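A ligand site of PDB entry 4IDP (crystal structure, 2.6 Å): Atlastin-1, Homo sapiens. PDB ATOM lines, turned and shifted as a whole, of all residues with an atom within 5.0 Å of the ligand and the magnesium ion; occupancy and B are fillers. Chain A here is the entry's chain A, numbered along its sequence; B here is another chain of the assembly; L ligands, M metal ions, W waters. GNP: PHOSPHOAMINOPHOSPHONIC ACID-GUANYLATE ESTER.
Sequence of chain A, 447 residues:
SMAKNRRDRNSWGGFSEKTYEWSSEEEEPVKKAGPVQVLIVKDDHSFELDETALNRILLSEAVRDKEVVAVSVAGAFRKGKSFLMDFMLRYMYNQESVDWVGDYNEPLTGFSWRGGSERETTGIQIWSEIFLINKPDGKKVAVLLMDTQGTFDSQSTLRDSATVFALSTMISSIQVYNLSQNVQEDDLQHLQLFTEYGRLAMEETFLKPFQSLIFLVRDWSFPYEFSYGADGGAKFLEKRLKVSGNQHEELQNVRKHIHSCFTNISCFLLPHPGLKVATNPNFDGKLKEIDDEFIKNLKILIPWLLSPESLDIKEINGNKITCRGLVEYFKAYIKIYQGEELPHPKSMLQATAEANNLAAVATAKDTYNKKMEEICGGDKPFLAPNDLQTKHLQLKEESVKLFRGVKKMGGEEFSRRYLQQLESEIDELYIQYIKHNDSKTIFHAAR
O2G of the ligand sits close to N of Thr 121, at 3.1 Å. N of Ser 82 lies within hydrogen-bond range of O2A of the ligand (3.2 Å). The backbone carbonyl oxygen (O) of Val 277 is in hydrogen-bond range of an oxygen (O2') of the ligand (2.7 Å). The backbone NH of Glu 120 is in hydrogen-bond range of an oxygen (O1G) of the ligand (2.7 Å). The backbone NH (N) of Arg 78 is in hydrogen-bond range of an oxygen (O3G) of the ligand (3.4 Å). An oxygen (O1G) of the ligand lies within salt-bridge range of the guanidinium group (NH1) of Arg 78, 2.7 Å away. An oxygen (O1B) of the ligand sits at hydrogen-bond distance from the backbone NH (N) of Lys 81, 2.9 Å away. NZ of Lys 81 lies within salt-bridge range of O1B of the ligand. N of Phe 83 lies within hydrogen-bond range of O2A of the ligand. The side-chain carboxylate (OD2) of Asp 219 is in hydrogen-bond range of a nitrogen (N2) of the ligand (2.9 Å). The backbone NH of Gly 80 lies within hydrogen-bond range of an oxygen (O3A) of the ligand (3.0 Å). NH2 of Arg 218 sits at hydrogen-bond distance from N7 of the ligand, at 3.0 Å. An oxygen (O1B) of the ligand lies within hydrogen-bond range of the backbone NH of Lys 79, at 3.2 Å. N of Gly 150 sits at hydrogen-bond distance from O3G of the ligand (3.5 Å).
The side-chain hydroxyl (OG) of Ser 82 sits close to the side-chain carboxylate (OD2) of Asp 147. The side-chain carboxylate (OE1) of Glu 120 is in hydrogen-bond range of the side-chain hydroxyl (OG) of Ser 112, 2.6 Å away. The guanidinium group (NH2) of Arg 78 sits at hydrogen-bond distance from the backbone carbonyl oxygen (O) of Gly 115 (3.3 Å). The guanidinium group (NE) of Arg 78 lies within hydrogen-bond range of the backbone carbonyl oxygen (O) of Glu 118 (3.4 Å). The backbone carbonyl oxygen (O) of Ala 76 lies within hydrogen-bond range of the side-chain amino group (NZ) of Lys 81, 2.9 Å away. NH2 of Arg 218 lies within hydrogen-bond range of O of Gly 80, 2.9 Å away. O of Arg 119 lies within hydrogen-bond range of NH2 of Arg 114, at 2.8 Å. O of Glu 118 sits at hydrogen-bond distance from NH1 of Arg 114 (2.8 Å).
CA of Phe 77 touches O3G of the ligand (3.4 Å). Trp 113 touches the ligand (CB to O1A, 3.4 Å). O of Arg 114 touches C5' of the ligand, 3.2 Å away. CA of Gly 115 touches O3' of the ligand (3.3 Å). Arg 119 touches the ligand. His 272 touches the ligand. Pro 273 touches the ligand (CD to N1, 3.2 Å). CE2 of Phe 283 touches O2' of the ligand, at 3.7 Å. Phe 294 touches the ligand (CE2 to O6, 3.9 Å). Hydrophobic or aromatic side chains within 4 Å of the ligand: Phe 77, Phe 83, Trp 113, His 272, Pro 273, Val 277, Phe 283 and Phe 294. Within 4 Å of the ligand: Phe 77, Arg 78, Lys 79, Gly 80, Lys 81, Ser 82, Phe 83, Trp 113, Arg 114, Gly 115, Arg 119, Glu 120, Thr 121, Gly 150, Arg 218, Asp 219, His 272, Pro 273, Val 277, Phe 283 and Phe 294.
Residues that only touch the magnesium ion: Asp 147 (3.9 Å). Three residues have an atom within 4 Å of the magnesium ion: Ser 82, Thr 121 and Asp 147.
The magnesium ion is bound by water W2 (1.8 Å), an oxygen (O2G) of the ligand (1.9 Å), water W1 (1.9 Å), an oxygen (O2B) of the ligand (2.1 Å), the side-chain hydroxyl (OG1) of Thr 121 (2.2 Å) and the side-chain hydroxyl (OG) of Ser 82 (2.2 Å).
Water W2 bridges O of Thr 148 (3.0 Å) and OD1 of Asp 147 (3.1 Å). Water W1 bridges an oxygen (O1A) of the ligand and the backbone carbonyl oxygen of Ser 112. Water W6 lies within hydrogen-bond range of an oxygen (O3') of the ligand (2.8 Å) and the backbone carbonyl oxygen of Ala 278 (2.8 Å). Water W3 lies within hydrogen-bond range of O of Thr 121 (2.7 Å), O3G of the ligand (2.9 Å) and N of Gly 150 (3.0 Å). Water W5 lies within hydrogen-bond range of O of Pro 271, N of Asp 219 and O6 of the ligand. Water W4 lies within hydrogen-bond range of O of Lys 79 (3.1 Å) and N1 of the ligand (3.3 Å).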
ATOM      1  N   ALA A  76      -7.635  11.442 -28.759  1.00  0.00           N
ATOM      2  CA  ALA A  76      -7.747  12.183 -27.505  1.00  0.00           C
ATOM      3  C   ALA A  76      -9.138  12.722 -27.237  1.00  0.00           C
ATOM      4  O   ALA A  76      -9.869  13.054 -28.154  1.00  0.00           O
ATOM      5  CB  ALA A  76      -6.752  13.308 -27.490  1.00  0.00           C
ATOM      6  N   PHE A  77      -9.534  12.750 -25.971  1.00  0.00           N
ATOM      7  CA  PHE A  77     -10.849  13.285 -25.623  1.00  0.00           C
ATOM      8  C   PHE A  77     -10.970  14.813 -25.874  1.00  0.00           C
ATOM      9  O   PHE A  77      -9.959  15.533 -25.906  1.00  0.00           O
ATOM     10  CB  PHE A  77     -11.285  12.864 -24.212  1.00  0.00           C
ATOM     11  CG  PHE A  77     -10.768  13.768 -23.135  1.00  0.00           C
ATOM     12  CD1 PHE A  77      -9.394  13.860 -22.906  1.00  0.00           C
ATOM     13  CD2 PHE A  77     -11.613  14.436 -22.286  1.00  0.00           C
ATOM     14  CE1 PHE A  77      -8.868  14.682 -21.907  1.00  0.00           C
ATOM     15  CE2 PHE A  77     -11.097  15.261 -21.270  1.00  0.00           C
ATOM     16  CZ  PHE A  77      -9.723  15.379 -21.091  1.00  0.00           C
ATOM     17  N   ARG A  78     -12.217  15.246 -26.068  1.00  0.00           N
ATOM     18  CA  ARG A  78     -12.621  16.635 -26.327  1.00  0.00           C
ATOM     19  C   ARG A  78     -12.085  17.229 -27.584  1.00  0.00           C
ATOM     20  O   ARG A  78     -11.851  18.415 -27.600  1.00  0.00           O
ATOM     21  CB  ARG A  78     -12.242  17.592 -25.173  1.00  0.00           C
ATOM     22  CG  ARG A  78     -12.746  17.261 -23.776  1.00  0.00           C
ATOM     23  CD  ARG A  78     -14.089  16.566 -23.823  1.00  0.00           C
ATOM     24  NE  ARG A  78     -15.147  17.511 -24.118  1.00  0.00           N
ATOM     25  CZ  ARG A  78     -16.292  17.209 -24.713  1.00  0.00           C
ATOM     26  NH1 ARG A  78     -16.551  15.968 -25.100  1.00  0.00           N
ATOM     27  NH2 ARG A  78     -17.189  18.164 -24.927  1.00  0.00           N
ATOM     28  N   LYS A  79     -11.897  16.451 -28.639  1.00  0.00           N
ATOM     29  CA  LYS A  79     -11.339  16.984 -29.865  1.00  0.00           C
ATOM     30  C   LYS A  79     -12.311  16.899 -31.082  1.00  0.00           C
ATOM     31  O   LYS A  79     -11.901  17.049 -32.256  1.00  0.00           O
ATOM     32  CB  LYS A  79      -9.985  16.350 -30.179  1.00  0.00           C
ATOM     33  CG  LYS A  79      -8.963  16.441 -29.015  1.00  0.00           C
ATOM     34  CD  LYS A  79      -8.557  17.878 -28.728  1.00  0.00           C
ATOM     35  CE  LYS A  79      -7.289  17.956 -27.908  1.00  0.00           C
ATOM     36  NZ  LYS A  79      -7.160  19.352 -27.347  1.00  0.00           N
ATOM     37  N   GLY A  80     -13.592  16.688 -30.801  1.00  0.00           N
ATOM     38  CA  GLY A  80     -14.602  16.684 -31.852  1.00  0.00           C
ATOM     39  C   GLY A  80     -14.861  15.441 -32.669  1.00  0.00           C
ATOM     40  O   GLY A  80     -15.202  15.523 -33.842  1.00  0.00           O
ATOM     41  N   LYS A  81     -14.646  14.299 -32.073  1.00  0.00           N
ATOM     42  CA  LYS A  81     -14.954  13.025 -32.706  1.00  0.00           C
ATOM     43  C   LYS A  81     -16.462  12.812 -32.964  1.00  0.00           C
ATOM     44  O   LYS A  81     -16.879  12.564 -34.094  1.00  0.00           O
ATOM     45  CB  LYS A  81     -14.342  11.857 -31.876  1.00  0.00           C
ATOM     46  CG  LYS A  81     -12.813  11.877 -31.758  1.00  0.00           C
ATOM     47  CD  LYS A  81     -12.196  10.716 -30.949  1.00  0.00           C
ATOM     48  CE  LYS A  81     -12.685  10.642 -29.458  1.00  0.00           C
ATOM     49  NZ  LYS A  81     -12.540  11.925 -28.676  1.00  0.00           N
ATOM     50  N   SER A  82     -17.275  12.984 -31.922  1.00  0.00           N
ATOM     51  CA  SER A  82     -18.707  12.740 -32.050  1.00  0.00           C
ATOM     52  C   SER A  82     -19.356  13.695 -33.039  1.00  0.00           C
ATOM     53  O   SER A  82     -20.216  13.305 -33.841  1.00  0.00           O
ATOM     54  CB  SER A  82     -19.394  12.883 -30.699  1.00  0.00           C
ATOM     55  OG  SER A  82     -19.022  11.856 -29.850  1.00  0.00           O
ATOM     56  N   PHE A  83     -18.874  14.928 -32.986  1.00  0.00           N
ATOM     57  CA  PHE A  83     -19.335  16.019 -33.824  1.00  0.00           C
ATOM     58  C   PHE A  83     -19.097  15.640 -35.303  1.00  0.00           C
ATOM     59  O   PHE A  83     -20.052  15.589 -36.096  1.00  0.00           O
ATOM     60  CB  PHE A  83     -18.553  17.261 -33.365  1.00  0.00           C
ATOM     61  CG  PHE A  83     -18.772  18.492 -34.195  1.00  0.00           C
ATOM     62  CD1 PHE A  83     -19.762  19.388 -33.853  1.00  0.00           C
ATOM     63  CD2 PHE A  83     -17.914  18.800 -35.244  1.00  0.00           C
ATOM     64  CE1 PHE A  83     -19.936  20.528 -34.588  1.00  0.00           C
ATOM     65  CE2 PHE A  83     -18.088  19.939 -35.979  1.00  0.00           C
ATOM     66  CZ  PHE A  83     -19.101  20.810 -35.659  1.00  0.00           C
ATOM     67  N   SER A 112     -23.969  11.790 -28.949  1.00  0.00           N
ATOM     68  CA  SER A 112     -23.962  12.940 -28.081  1.00  0.00           C
ATOM     69  C   SER A 112     -22.627  13.714 -28.071  1.00  0.00           C
ATOM     70  O   SER A 112     -21.544  13.133 -28.002  1.00  0.00           O
ATOM     71  CB  SER A 112     -24.374  12.522 -26.667  1.00  0.00           C
ATOM     72  OG  SER A 112     -24.270  13.606 -25.770  1.00  0.00           O
ATOM     73  N   TRP A 113     -22.698  15.011 -28.312  1.00  0.00           N
ATOM     74  CA  TRP A 113     -21.531  15.913 -28.322  1.00  0.00           C
ATOM     75  C   TRP A 113     -21.916  17.219 -27.606  1.00  0.00           C
ATOM     76  O   TRP A 113     -23.108  17.563 -27.526  1.00  0.00           O
ATOM     77  CB  TRP A 113     -21.059  16.177 -29.764  1.00  0.00           C
ATOM     78  CG  TRP A 113     -21.989  17.011 -30.565  1.00  0.00           C
ATOM     79  CD1 TRP A 113     -23.064  16.581 -31.254  1.00  0.00           C
ATOM     80  CD2 TRP A 113     -21.933  18.439 -30.748  1.00  0.00           C
ATOM     81  NE1 TRP A 113     -23.688  17.640 -31.869  1.00  0.00           N
ATOM     82  CE2 TRP A 113     -23.017  18.789 -31.569  1.00  0.00           C
ATOM     83  CE3 TRP A 113     -21.090  19.455 -30.285  1.00  0.00           C
ATOM     84  CZ2 TRP A 113     -23.273  20.107 -31.954  1.00  0.00           C
ATOM     85  CZ3 TRP A 113     -21.341  20.766 -30.666  1.00  0.00           C
ATOM     86  CH2 TRP A 113     -22.426  21.073 -31.495  1.00  0.00           C
ATOM     87  N   ARG A 114     -20.920  17.903 -27.051  1.00  0.00           N
ATOM     88  CA  ARG A 114     -21.123  19.178 -26.343  1.00  0.00           C
ATOM     89  C   ARG A 114     -19.762  19.825 -26.047  1.00  0.00           C
ATOM     90  O   ARG A 114     -18.721  19.202 -26.253  1.00  0.00           O
ATOM     91  CB  ARG A 114     -21.904  18.992 -25.031  1.00  0.00           C
ATOM     92  CG  ARG A 114     -21.318  17.903 -24.109  1.00  0.00           C
ATOM     93  CD  ARG A 114     -21.453  18.143 -22.600  1.00  0.00           C
ATOM     94  NE  ARG A 114     -20.889  17.018 -21.861  1.00  0.00           N
ATOM     95  CZ  ARG A 114     -19.618  16.907 -21.471  1.00  0.00           C
ATOM     96  NH1 ARG A 114     -18.756  17.891 -21.714  1.00  0.00           N
ATOM     97  NH2 ARG A 114     -19.223  15.830 -20.812  1.00  0.00           N
ATOM     98  N   GLY A 115     -19.768  21.076 -25.617  1.00  0.00           N
ATOM     99  CA  GLY A 115     -18.563  21.730 -25.157  1.00  0.00           C
ATOM    100  C   GLY A 115     -18.291  21.343 -23.711  1.00  0.00           C
ATOM    101  O   GLY A 115     -18.886  20.391 -23.212  1.00  0.00           O
ATOM    102  N   GLU A 118     -14.962  18.357 -19.613  1.00  0.00           N
ATOM    103  CA  GLU A 118     -15.148  16.963 -19.161  1.00  0.00           C
ATOM    104  C   GLU A 118     -15.594  16.067 -20.314  1.00  0.00           C
ATOM    105  O   GLU A 118     -16.406  16.464 -21.146  1.00  0.00           O
ATOM    106  CB  GLU A 118     -16.136  16.873 -17.992  1.00  0.00           C
ATOM    107  CG  GLU A 118     -15.695  17.721 -16.802  1.00  0.00           C
ATOM    108  CD  GLU A 118     -14.438  17.174 -16.113  1.00  0.00           C
ATOM    109  OE1 GLU A 118     -14.377  15.943 -15.851  1.00  0.00           O
ATOM    110  OE2 GLU A 118     -13.490  17.989 -15.890  1.00  0.00           O
ATOM    111  N   ARG A 119     -14.985  14.882 -20.344  1.00  0.00           N
ATOM    112  CA  ARG A 119     -15.260  13.888 -21.363  1.00  0.00           C
ATOM    113  C   ARG A 119     -16.744  13.625 -21.438  1.00  0.00           C
ATOM    114  O   ARG A 119     -17.451  13.678 -20.437  1.00  0.00           O
ATOM    115  CB  ARG A 119     -14.556  12.565 -21.089  1.00  0.00           C
ATOM    116  CG  ARG A 119     -15.177  11.803 -19.942  1.00  0.00           C
ATOM    117  CD  ARG A 119     -14.556  10.467 -19.935  1.00  0.00           C
ATOM    118  NE  ARG A 119     -15.066   9.504 -18.955  1.00  0.00           N
ATOM    119  CZ  ARG A 119     -14.423   8.362 -18.727  1.00  0.00           C
ATOM    120  NH1 ARG A 119     -13.335   8.036 -19.463  1.00  0.00           N
ATOM    121  NH2 ARG A 119     -14.897   7.520 -17.833  1.00  0.00           N
ATOM    122  N   GLU A 120     -17.195  13.274 -22.635  1.00  0.00           N
ATOM    123  CA  GLU A 120     -18.571  12.874 -22.898  1.00  0.00           C
ATOM    124  C   GLU A 120     -18.777  11.387 -23.284  1.00  0.00           C
ATOM    125  O   GLU A 120     -19.402  10.654 -22.526  1.00  0.00           O
ATOM    126  CB  GLU A 120     -19.124  13.847 -23.973  1.00  0.00           C
ATOM    127  CG  GLU A 120     -20.498  13.527 -24.524  1.00  0.00           C
ATOM    128  CD  GLU A 120     -21.572  13.541 -23.475  1.00  0.00           C
ATOM    129  OE1 GLU A 120     -22.695  13.056 -23.767  1.00  0.00           O
ATOM    130  OE2 GLU A 120     -21.356  14.116 -22.383  1.00  0.00           O
ATOM    131  N   THR A 121     -18.311  10.955 -24.450  1.00  0.00           N
ATOM    132  CA  THR A 121     -18.476   9.575 -24.906  1.00  0.00           C
ATOM    133  C   THR A 121     -17.691   8.587 -24.055  1.00  0.00           C
ATOM    134  O   THR A 121     -16.525   8.778 -23.773  1.00  0.00           O
ATOM    135  CB  THR A 121     -18.018   9.425 -26.320  1.00  0.00           C
ATOM    136  OG1 THR A 121     -18.659  10.434 -27.101  1.00  0.00           O
ATOM    137  CG2 THR A 121     -18.419   8.047 -26.867  1.00  0.00           C
ATOM    138  N   ASP A 147     -18.473   5.160 -32.590  1.00  0.00           N
ATOM    139  CA  ASP A 147     -17.906   6.279 -31.846  1.00  0.00           C
ATOM    140  C   ASP A 147     -17.321   5.829 -30.536  1.00  0.00           C
ATOM    141  O   ASP A 147     -17.943   5.059 -29.806  1.00  0.00           O
ATOM    142  CB  ASP A 147     -18.989   7.332 -31.611  1.00  0.00           C
ATOM    143  CG  ASP A 147     -18.420   8.646 -31.099  1.00  0.00           C
ATOM    144  OD1 ASP A 147     -17.222   8.950 -31.369  1.00  0.00           O
ATOM    145  OD2 ASP A 147     -19.204   9.434 -30.531  1.00  0.00           O
ATOM    146  N   THR A 148     -16.196   6.402 -30.171  1.00  0.00           N
ATOM    147  CA  THR A 148     -15.389   5.859 -29.104  1.00  0.00           C
ATOM    148  C   THR A 148     -15.066   6.875 -28.048  1.00  0.00           C
ATOM    149  O   THR A 148     -14.985   8.052 -28.338  1.00  0.00           O
ATOM    150  CB  THR A 148     -14.064   5.262 -29.624  1.00  0.00           C
ATOM    151  OG1 THR A 148     -13.188   6.342 -29.975  1.00  0.00           O
ATOM    152  CG2 THR A 148     -14.324   4.397 -30.870  1.00  0.00           C
ATOM    153  N   GLN A 149     -14.807   6.398 -26.854  1.00  0.00           N
ATOM    154  CA  GLN A 149     -14.360   7.178 -25.733  1.00  0.00           C
ATOM    155  C   GLN A 149     -12.932   7.759 -25.984  1.00  0.00           C
ATOM    156  O   GLN A 149     -12.021   7.053 -26.464  1.00  0.00           O
ATOM    157  CB  GLN A 149     -14.388   6.312 -24.508  1.00  0.00           C
ATOM    158  CG  GLN A 149     -13.732   6.810 -23.268  1.00  0.00           C
ATOM    159  CD  GLN A 149     -13.842   5.821 -22.088  1.00  0.00           C
ATOM    160  OE1 GLN A 149     -14.777   5.075 -21.996  1.00  0.00           O
ATOM    161  NE2 GLN A 149     -12.771   5.739 -21.247  1.00  0.00           N
ATOM    162  N   GLY A 150     -12.782   9.059 -25.760  1.00  0.00           N
ATOM    163  CA  GLY A 150     -11.508   9.694 -25.989  1.00  0.00           C
ATOM    164  C   GLY A 150     -10.407   9.193 -25.082  1.00  0.00           C
ATOM    165  O   GLY A 150     -10.642   8.927 -23.897  1.00  0.00           O
ATOM    166  N   ARG A 218      -7.144  18.137 -36.922  1.00  0.00           N
ATOM    167  CA  ARG A 218      -8.083  19.231 -36.655  1.00  0.00           C
ATOM    168  C   ARG A 218      -7.288  20.487 -36.423  1.00  0.00           C
ATOM    169  O   ARG A 218      -6.207  20.419 -35.858  1.00  0.00           O
ATOM    170  CB  ARG A 218      -8.973  18.932 -35.440  1.00  0.00           C
ATOM    171  CG  ARG A 218      -9.566  17.560 -35.483  1.00  0.00           C
ATOM    172  CD  ARG A 218     -10.591  17.435 -36.609  1.00  0.00           C
ATOM    173  NE  ARG A 218     -11.882  17.974 -36.202  1.00  0.00           N
ATOM    174  CZ  ARG A 218     -12.847  17.221 -35.685  1.00  0.00           C
ATOM    175  NH1 ARG A 218     -12.661  15.910 -35.516  1.00  0.00           N
ATOM    176  NH2 ARG A 218     -14.011  17.738 -35.330  1.00  0.00           N
ATOM    177  N   ASP A 219      -7.856  21.635 -36.818  1.00  0.00           N
ATOM    178  CA  ASP A 219      -7.241  22.936 -36.580  1.00  0.00           C
ATOM    179  C   ASP A 219      -5.850  23.036 -37.156  1.00  0.00           C
ATOM    180  O   ASP A 219      -4.979  23.649 -36.536  1.00  0.00           O
ATOM    181  CB  ASP A 219      -7.202  23.269 -35.074  1.00  0.00           C
ATOM    182  CG  ASP A 219      -8.538  23.140 -34.416  1.00  0.00           C
ATOM    183  OD1 ASP A 219      -9.542  23.077 -35.143  1.00  0.00           O
ATOM    184  OD2 ASP A 219      -8.594  23.147 -33.182  1.00  0.00           O
ATOM    185  N   PRO A 271      -9.213  22.615 -41.534  1.00  0.00           N
ATOM    186  CA  PRO A 271      -9.039  23.919 -40.877  1.00  0.00           C
ATOM    187  C   PRO A 271      -9.810  24.033 -39.560  1.00  0.00           C
ATOM    188  O   PRO A 271     -10.712  23.248 -39.352  1.00  0.00           O
ATOM    189  CB  PRO A 271      -9.556  24.945 -41.915  1.00  0.00           C
ATOM    190  CG  PRO A 271     -10.328  24.163 -42.910  1.00  0.00           C
ATOM    191  CD  PRO A 271      -9.891  22.708 -42.834  1.00  0.00           C
ATOM    192  N   HIS A 272      -9.454  25.002 -38.724  1.00  0.00           N
ATOM    193  CA  HIS A 272     -10.240  25.373 -37.539  1.00  0.00           C
ATOM    194  C   HIS A 272     -11.703  25.752 -37.968  1.00  0.00           C
ATOM    195  O   HIS A 272     -11.937  26.378 -39.014  1.00  0.00           O
ATOM    196  CB  HIS A 272      -9.595  26.579 -36.818  1.00  0.00           C
ATOM    197  CG  HIS A 272      -9.995  26.740 -35.373  1.00  0.00           C
ATOM    198  ND1 HIS A 272     -11.271  27.091 -34.957  1.00  0.00           N
ATOM    199  CD2 HIS A 272      -9.248  26.647 -34.242  1.00  0.00           C
ATOM    200  CE1 HIS A 272     -11.295  27.173 -33.633  1.00  0.00           C
ATOM    201  NE2 HIS A 272     -10.080  26.908 -33.175  1.00  0.00           N
ATOM    202  N   PRO A 273     -12.711  25.283 -37.196  1.00  0.00           N
ATOM    203  CA  PRO A 273     -14.093  25.599 -37.570  1.00  0.00           C
ATOM    204  C   PRO A 273     -14.525  26.993 -37.114  1.00  0.00           C
ATOM    205  O   PRO A 273     -15.687  27.347 -37.318  1.00  0.00           O
ATOM    206  CB  PRO A 273     -14.911  24.510 -36.859  1.00  0.00           C
ATOM    207  CG  PRO A 273     -14.044  24.111 -35.647  1.00  0.00           C
ATOM    208  CD  PRO A 273     -12.600  24.313 -36.076  1.00  0.00           C
ATOM    209  N   VAL A 277     -17.607  27.820 -32.794  1.00  0.00           N
ATOM    210  CA  VAL A 277     -17.691  26.361 -32.613  1.00  0.00           C
ATOM    211  C   VAL A 277     -16.915  25.935 -31.368  1.00  0.00           C
ATOM    212  O   VAL A 277     -17.379  25.097 -30.586  1.00  0.00           O
ATOM    213  CB  VAL A 277     -17.145  25.620 -33.870  1.00  0.00           C
ATOM    214  CG1 VAL A 277     -17.040  24.080 -33.651  1.00  0.00           C
ATOM    215  CG2 VAL A 277     -18.016  25.926 -35.086  1.00  0.00           C
ATOM    216  N   ALA A 278     -15.731  26.501 -31.200  1.00  0.00           N
ATOM    217  CA  ALA A 278     -14.831  26.209 -30.098  1.00  0.00           C
ATOM    218  C   ALA A 278     -15.296  26.753 -28.723  1.00  0.00           C
ATOM    219  O   ALA A 278     -15.138  26.103 -27.683  1.00  0.00           O
ATOM    220  CB  ALA A 278     -13.384  26.693 -30.419  1.00  0.00           C
ATOM    221  N   PHE A 283     -23.577  27.119 -28.947  1.00  0.00           N
ATOM    222  CA  PHE A 283     -23.502  26.462 -30.268  1.00  0.00           C
ATOM    223  C   PHE A 283     -24.019  25.005 -30.349  1.00  0.00           C
ATOM    224  O   PHE A 283     -23.616  24.173 -29.529  1.00  0.00           O
ATOM    225  CB  PHE A 283     -22.047  26.517 -30.754  1.00  0.00           C
ATOM    226  CG  PHE A 283     -21.750  25.717 -31.999  1.00  0.00           C
ATOM    227  CD1 PHE A 283     -22.298  26.034 -33.237  1.00  0.00           C
ATOM    228  CD2 PHE A 283     -20.889  24.615 -31.915  1.00  0.00           C
ATOM    229  CE1 PHE A 283     -21.981  25.284 -34.348  1.00  0.00           C
ATOM    230  CE2 PHE A 283     -20.572  23.865 -33.026  1.00  0.00           C
ATOM    231  CZ  PHE A 283     -21.121  24.203 -34.245  1.00  0.00           C
ATOM    232  N   PHE A 294     -13.887  25.659 -43.315  1.00  0.00           N
ATOM    233  CA  PHE A 294     -14.103  24.382 -42.686  1.00  0.00           C
ATOM    234  C   PHE A 294     -15.194  23.588 -43.400  1.00  0.00           C
ATOM    235  O   PHE A 294     -15.023  22.399 -43.672  1.00  0.00           O
ATOM    236  CB  PHE A 294     -14.467  24.567 -41.211  1.00  0.00           C
ATOM    237  CG  PHE A 294     -14.797  23.290 -40.461  1.00  0.00           C
ATOM    238  CD1 PHE A 294     -16.080  22.742 -40.514  1.00  0.00           C
ATOM    239  CD2 PHE A 294     -13.839  22.666 -39.681  1.00  0.00           C
ATOM    240  CE1 PHE A 294     -16.405  21.614 -39.803  1.00  0.00           C
ATOM    241  CE2 PHE A 294     -14.154  21.529 -38.974  1.00  0.00           C
ATOM    242  CZ  PHE A 294     -15.440  21.003 -39.031  1.00  0.00           C
ATOM    243  N   GLN B 181      -4.873  23.845 -25.026  1.00  0.00           N
ATOM    244  CA  GLN B 181      -6.334  23.597 -24.857  1.00  0.00           C
ATOM    245  C   GLN B 181      -6.762  22.922 -23.538  1.00  0.00           C
ATOM    246  O   GLN B 181      -7.818  23.231 -23.014  1.00  0.00           O
ATOM    247  CB  GLN B 181      -6.930  22.748 -26.010  1.00  0.00           C
ATOM    248  CG  GLN B 181      -6.919  23.419 -27.384  1.00  0.00           C
ATOM    249  CD  GLN B 181      -7.304  22.442 -28.492  1.00  0.00           C
ATOM    250  OE1 GLN B 181      -6.526  21.574 -28.821  1.00  0.00           O
ATOM    251  NE2 GLN B 181      -8.431  22.695 -29.141  1.00  0.00           N
HETATM  252  PG  GNP L   1     -15.307  13.036 -26.113  1.00  0.00           P
HETATM  253  O1G GNP L   1     -15.414  13.514 -24.674  1.00  0.00           O
HETATM  254  O2G GNP L   1     -16.451  12.255 -26.627  1.00  0.00           O
HETATM  255  O3G GNP L   1     -13.979  12.294 -26.301  1.00  0.00           O
HETATM  256  N3B GNP L   1     -15.289  14.355 -27.013  1.00  0.00           N
HETATM  257  PB  GNP L   1     -15.327  14.414 -28.600  1.00  0.00           P
HETATM  258  O1B GNP L   1     -14.013  14.189 -29.229  1.00  0.00           O
HETATM  259  O2B GNP L   1     -16.343  13.476 -29.103  1.00  0.00           O
HETATM  260  O3A GNP L   1     -15.726  15.865 -28.921  1.00  0.00           O
HETATM  261  PA  GNP L   1     -17.126  16.420 -29.300  1.00  0.00           P
HETATM  262  O1A GNP L   1     -18.047  16.182 -28.156  1.00  0.00           O
HETATM  263  O2A GNP L   1     -17.502  15.924 -30.633  1.00  0.00           O
HETATM  264  O5' GNP L   1     -16.848  17.978 -29.391  1.00  0.00           O
HETATM  265  C5' GNP L   1     -16.361  18.759 -28.295  1.00  0.00           C
HETATM  266  C4' GNP L   1     -16.251  20.246 -28.638  1.00  0.00           C
HETATM  267  O4' GNP L   1     -15.375  20.355 -29.781  1.00  0.00           O
HETATM  268  C3' GNP L   1     -17.535  20.982 -29.052  1.00  0.00           C
HETATM  269  O3' GNP L   1     -17.730  22.191 -28.332  1.00  0.00           O
HETATM  270  C2' GNP L   1     -17.313  21.280 -30.527  1.00  0.00           C
HETATM  271  O2' GNP L   1     -17.891  22.501 -30.914  1.00  0.00           O
HETATM  272  C1' GNP L   1     -15.804  21.414 -30.597  1.00  0.00           C
HETATM  273  N9  GNP L   1     -15.228  21.111 -31.901  1.00  0.00           N
HETATM  274  C8  GNP L   1     -15.738  20.258 -32.852  1.00  0.00           C
HETATM  275  N7  GNP L   1     -15.007  20.171 -33.928  1.00  0.00           N
HETATM  276  C5  GNP L   1     -13.929  21.001 -33.655  1.00  0.00           C
HETATM  277  C6  GNP L   1     -12.786  21.296 -34.433  1.00  0.00           C
HETATM  278  O6  GNP L   1     -12.459  20.888 -35.555  1.00  0.00           O
HETATM  279  N1  GNP L   1     -11.959  22.176 -33.755  1.00  0.00           N
HETATM  280  C2  GNP L   1     -12.183  22.719 -32.531  1.00  0.00           C
HETATM  281  N2  GNP L   1     -11.248  23.555 -32.087  1.00  0.00           N
HETATM  282  N3  GNP L   1     -13.234  22.437 -31.794  1.00  0.00           N
HETATM  283  C4  GNP L   1     -14.052  21.578 -32.412  1.00  0.00           C
HETATM  284 MG    MG M   1     -17.557  12.027 -28.184  1.00  0.00          MG
HETATM  285  O   HOH W   1     -18.649  13.540 -27.636  1.00  0.00           O
HETATM  286  O   HOH W   2     -16.594  10.557 -28.741  1.00  0.00           O
HETATM  287  O   HOH W   3     -14.516  10.634 -23.930  1.00  0.00           O
HETATM  288  O   HOH W   4     -10.638  19.817 -31.792  1.00  0.00           O
HETATM  289  O   HOH W   5     -10.443  21.080 -37.708  1.00  0.00           O
HETATM  290  O   HOH W   6     -15.171  23.318 -28.095  1.00  0.00           O
